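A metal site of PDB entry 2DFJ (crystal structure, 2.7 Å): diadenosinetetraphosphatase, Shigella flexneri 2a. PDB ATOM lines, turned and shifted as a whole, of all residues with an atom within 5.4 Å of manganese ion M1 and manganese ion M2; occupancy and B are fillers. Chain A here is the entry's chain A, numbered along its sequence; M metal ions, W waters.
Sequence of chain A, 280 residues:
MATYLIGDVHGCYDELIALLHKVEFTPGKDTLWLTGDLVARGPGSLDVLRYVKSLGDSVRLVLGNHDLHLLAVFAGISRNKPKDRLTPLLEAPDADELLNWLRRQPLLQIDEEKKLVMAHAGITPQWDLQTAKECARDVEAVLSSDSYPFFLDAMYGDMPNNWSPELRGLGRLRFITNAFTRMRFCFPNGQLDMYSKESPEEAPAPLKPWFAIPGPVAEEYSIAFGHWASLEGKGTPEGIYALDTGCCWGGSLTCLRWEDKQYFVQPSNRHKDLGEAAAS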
ATOM      1  N   ASP A   8     -10.743 -32.872  15.420  1.00  0.00           N
ATOM      2  CA  ASP A   8     -11.700 -32.094  16.229  1.00  0.00           C
ATOM      3  C   ASP A   8     -12.903 -32.849  16.742  1.00  0.00           C
ATOM      4  O   ASP A   8     -13.734 -33.325  15.958  1.00  0.00           O
ATOM      5  CB  ASP A   8     -12.154 -30.856  15.463  1.00  0.00           C
ATOM      6  CG  ASP A   8     -11.070 -29.823  15.350  1.00  0.00           C
ATOM      7  OD1 ASP A   8      -9.905 -30.213  15.522  1.00  0.00           O
ATOM      8  OD2 ASP A   8     -11.360 -28.643  15.113  1.00  0.00           O
ATOM      9  N   HIS A  10     -15.804 -31.975  18.421  1.00  0.00           N
ATOM     10  CA  HIS A  10     -16.586 -30.869  18.949  1.00  0.00           C
ATOM     11  C   HIS A  10     -17.727 -31.337  19.820  1.00  0.00           C
ATOM     12  O   HIS A  10     -18.834 -31.551  19.335  1.00  0.00           O
ATOM     13  CB  HIS A  10     -17.102 -30.021  17.821  1.00  0.00           C
ATOM     14  CG  HIS A  10     -16.057 -29.085  17.283  1.00  0.00           C
ATOM     15  ND1 HIS A  10     -15.572 -28.010  18.045  1.00  0.00           N
ATOM     16  CD2 HIS A  10     -15.388 -29.052  16.097  1.00  0.00           C
ATOM     17  CE1 HIS A  10     -14.718 -27.336  17.381  1.00  0.00           C
ATOM     18  NE2 HIS A  10     -14.525 -27.957  16.147  1.00  0.00           N
ATOM     19  N   ASP A  37      -9.948 -28.545  20.189  1.00  0.00           N
ATOM     20  CA  ASP A  37     -11.370 -28.259  19.961  1.00  0.00           C
ATOM     21  C   ASP A  37     -12.211 -29.447  20.409  1.00  0.00           C
ATOM     22  O   ASP A  37     -12.972 -30.036  19.642  1.00  0.00           O
ATOM     23  CB  ASP A  37     -11.655 -27.855  18.511  1.00  0.00           C
ATOM     24  CG  ASP A  37     -11.336 -26.400  18.230  1.00  0.00           C
ATOM     25  OD1 ASP A  37     -10.912 -25.669  19.161  1.00  0.00           O
ATOM     26  OD2 ASP A  37     -11.490 -25.970  17.064  1.00  0.00           O
ATOM     27  N   ARG A  41     -19.350 -27.267  19.161  1.00  0.00           N
ATOM     28  CA  ARG A  41     -20.791 -27.110  18.881  1.00  0.00           C
ATOM     29  C   ARG A  41     -21.673 -28.239  19.360  1.00  0.00           C
ATOM     30  O   ARG A  41     -22.815 -28.006  19.733  1.00  0.00           O
ATOM     31  CB  ARG A  41     -21.083 -26.885  17.389  1.00  0.00           C
ATOM     32  CG  ARG A  41     -20.102 -25.994  16.618  1.00  0.00           C
ATOM     33  CD  ARG A  41     -20.060 -24.532  17.130  1.00  0.00           C
ATOM     34  NE  ARG A  41     -19.158 -23.654  16.363  1.00  0.00           N
ATOM     35  CZ  ARG A  41     -18.013 -24.008  15.746  1.00  0.00           C
ATOM     36  NH1 ARG A  41     -17.544 -25.273  15.792  1.00  0.00           N
ATOM     37  NH2 ARG A  41     -17.315 -23.078  15.087  1.00  0.00           N
ATOM     38  N   GLY A  64      -7.087 -26.112  21.028  1.00  0.00           N
ATOM     39  CA  GLY A  64      -7.563 -25.355  19.859  1.00  0.00           C
ATOM     40  C   GLY A  64      -8.190 -24.006  20.199  1.00  0.00           C
ATOM     41  O   GLY A  64      -8.308 -23.633  21.379  1.00  0.00           O
ATOM     42  N   ASN A  65      -8.597 -23.263  19.159  1.00  0.00           N
ATOM     43  CA  ASN A  65      -9.250 -21.959  19.339  1.00  0.00           C
ATOM     44  C   ASN A  65     -10.488 -22.001  20.225  1.00  0.00           C
ATOM     45  O   ASN A  65     -10.681 -21.128  21.073  1.00  0.00           O
ATOM     46  CB  ASN A  65      -9.570 -21.315  17.976  1.00  0.00           C
ATOM     47  CG  ASN A  65     -10.255 -22.298  17.007  1.00  0.00           C
ATOM     48  OD1 ASN A  65      -9.765 -23.404  16.791  1.00  0.00           O
ATOM     49  ND2 ASN A  65     -11.365 -21.871  16.407  1.00  0.00           N
ATOM     50  N   HIS A  66     -11.330 -23.018  20.042  1.00  0.00           N
ATOM     51  CA  HIS A  66     -12.527 -23.163  20.876  1.00  0.00           C
ATOM     52  C   HIS A  66     -12.248 -23.545  22.329  1.00  0.00           C
ATOM     53  O   HIS A  66     -13.006 -23.164  23.217  1.00  0.00           O
ATOM     54  CB  HIS A  66     -13.509 -24.156  20.278  1.00  0.00           C
ATOM     55  CG  HIS A  66     -14.222 -23.621  19.074  1.00  0.00           C
ATOM     56  ND1 HIS A  66     -13.681 -23.673  17.809  1.00  0.00           N
ATOM     57  CD2 HIS A  66     -15.428 -23.017  18.957  1.00  0.00           C
ATOM     58  CE1 HIS A  66     -14.532 -23.132  16.955  1.00  0.00           C
ATOM     59  NE2 HIS A  66     -15.600 -22.735  17.620  1.00  0.00           N
ATOM     60  N   HIS A 120      -2.647 -27.623  16.856  1.00  0.00           N
ATOM     61  CA  HIS A 120      -4.048 -27.561  16.444  1.00  0.00           C
ATOM     62  C   HIS A 120      -4.262 -27.186  14.975  1.00  0.00           C
ATOM     63  O   HIS A 120      -4.971 -27.891  14.266  1.00  0.00           O
ATOM     64  CB  HIS A 120      -4.853 -26.636  17.346  1.00  0.00           C
ATOM     65  CG  HIS A 120      -6.295 -26.517  16.950  1.00  0.00           C
ATOM     66  ND1 HIS A 120      -7.169 -27.579  16.973  1.00  0.00           N
ATOM     67  CD2 HIS A 120      -7.019 -25.448  16.533  1.00  0.00           C
ATOM     68  CE1 HIS A 120      -8.369 -27.179  16.603  1.00  0.00           C
ATOM     69  NE2 HIS A 120      -8.302 -25.887  16.334  1.00  0.00           N
ATOM     70  N   THR A 181      -3.407 -21.897  16.513  1.00  0.00           N
ATOM     71  CA  THR A 181      -4.835 -22.185  16.681  1.00  0.00           C
ATOM     72  C   THR A 181      -5.813 -21.547  15.688  1.00  0.00           C
ATOM     73  O   THR A 181      -7.013 -21.838  15.750  1.00  0.00           O
ATOM     74  CB  THR A 181      -5.331 -21.875  18.122  1.00  0.00           C
ATOM     75  OG1 THR A 181      -5.439 -20.464  18.317  1.00  0.00           O
ATOM     76  CG2 THR A 181      -4.388 -22.442  19.165  1.00  0.00           C
ATOM     77  N   GLY A 226      -5.627 -30.333  12.896  1.00  0.00           N
ATOM     78  CA  GLY A 226      -7.031 -30.410  12.500  1.00  0.00           C
ATOM     79  C   GLY A 226      -7.873 -29.235  12.927  1.00  0.00           C
ATOM     80  O   GLY A 226      -8.593 -29.309  13.907  1.00  0.00           O
ATOM     81  N   HIS A 227      -7.807 -28.138  12.208  1.00  0.00           N
ATOM     82  CA  HIS A 227      -8.609 -26.988  12.563  1.00  0.00           C
ATOM     83  C   HIS A 227      -9.389 -26.671  11.305  1.00  0.00           C
ATOM     84  O   HIS A 227     -10.609 -26.522  11.313  1.00  0.00           O
ATOM     85  CB  HIS A 227      -7.673 -25.863  13.014  1.00  0.00           C
ATOM     86  CG  HIS A 227      -8.243 -24.483  12.884  1.00  0.00           C
ATOM     87  ND1 HIS A 227      -9.368 -24.068  13.572  1.00  0.00           N
ATOM     88  CD2 HIS A 227      -7.782 -23.399  12.193  1.00  0.00           C
ATOM     89  CE1 HIS A 227      -9.607 -22.799  13.280  1.00  0.00           C
ATOM     90  NE2 HIS A 227      -8.655 -22.362  12.447  1.00  0.00           N
ATOM     91  N   ASP A 244      -9.163 -33.133  10.763  1.00  0.00           N
ATOM     92  CA  ASP A 244     -10.469 -32.497  10.986  1.00  0.00           C
ATOM     93  C   ASP A 244     -11.425 -32.673   9.800  1.00  0.00           C
ATOM     94  O   ASP A 244     -11.248 -32.068   8.726  1.00  0.00           O
ATOM     95  CB  ASP A 244     -10.321 -31.020  11.322  1.00  0.00           C
ATOM     96  CG  ASP A 244     -11.608 -30.406  11.852  1.00  0.00           C
ATOM     97  OD1 ASP A 244     -12.702 -30.998  11.675  1.00  0.00           O
ATOM     98  OD2 ASP A 244     -11.521 -29.311  12.442  1.00  0.00           O
HETATM   99 MN    MN M   1     -10.092 -24.956  15.414  1.00  0.00          MN
HETATM  100 MN    MN M   2     -12.806 -27.012  15.333  1.00  0.00          MN
HETATM  101  O   HOH W   1     -14.339 -25.046  14.953  1.00  0.00           O
HETATM  102  O   HOH W   2     -13.795 -28.144  13.630  1.00  0.00           O
HETATM  103  O   HOH W   3     -12.070 -24.010  14.754  1.00  0.00           O
HETATM  104  O   HOH W   4     -11.471 -26.402  14.049  1.00  0.00           O
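Asp 244 touches manganese ion M2.
Of the 12 residues printed, 4 come within 4 Å of manganese ion M2.
ND2 of Asn 65 lies within hydrogen-bond range of ND1 of His 66.
The side-chain amide oxygen of Asn 65 lies close to the backbone carbonyl oxygen of Thr 181, at 3.3 Å.
The backbone carbonyl oxygen (O) of His 120 lies within hydrogen-bond range of the backbone NH (N) of Gly 226, at 2.9 Å.
OD1 of Asp 37 lies within hydrogen-bond range of N of His 66 (2.8 Å).
Of the 12 residues printed, 5 come within 4 Å of manganese ion M1.
The nearest printed residue that does not touch manganese ion M1 is Thr 181 (4.4 Å).
Manganese ion M1 is bound by the side-chain amide oxygen of Asn 65 (2.1 Å), a ring nitrogen (ND1) of His 227 (2.2 Å), a ring nitrogen (NE2) of His 120 (2.2 Å), water W3 (2.3 Å), the side-chain carboxylate of Asp 37 (2.4 Å) and water W4 (2.4 Å).
Manganese ion M2 is bound by water W4, a ring nitrogen (NE2) of His 10, the side-chain carboxylate (OD2) of Asp 8, water W2, the side-chain carboxylate (OD2) of Asp 37 and water W1.
Manganese ion M2 has six donor atoms within binding distance.
Water W3 bridges the side-chain amide nitrogen of Asn 65 (2.8 Å) and a ring nitrogen (ND1) of His 66 (3.5 Å).
Water W4 lies within hydrogen-bond range of the backbone carbonyl oxygen (O) of His 227 and the side-chain carboxylate (OD2) of Asp 244.
Water W1 bridges a ring nitrogen (ND1) of His 66 (3.2 Å) and the guanidinium group of Arg 41 (3.3 Å).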
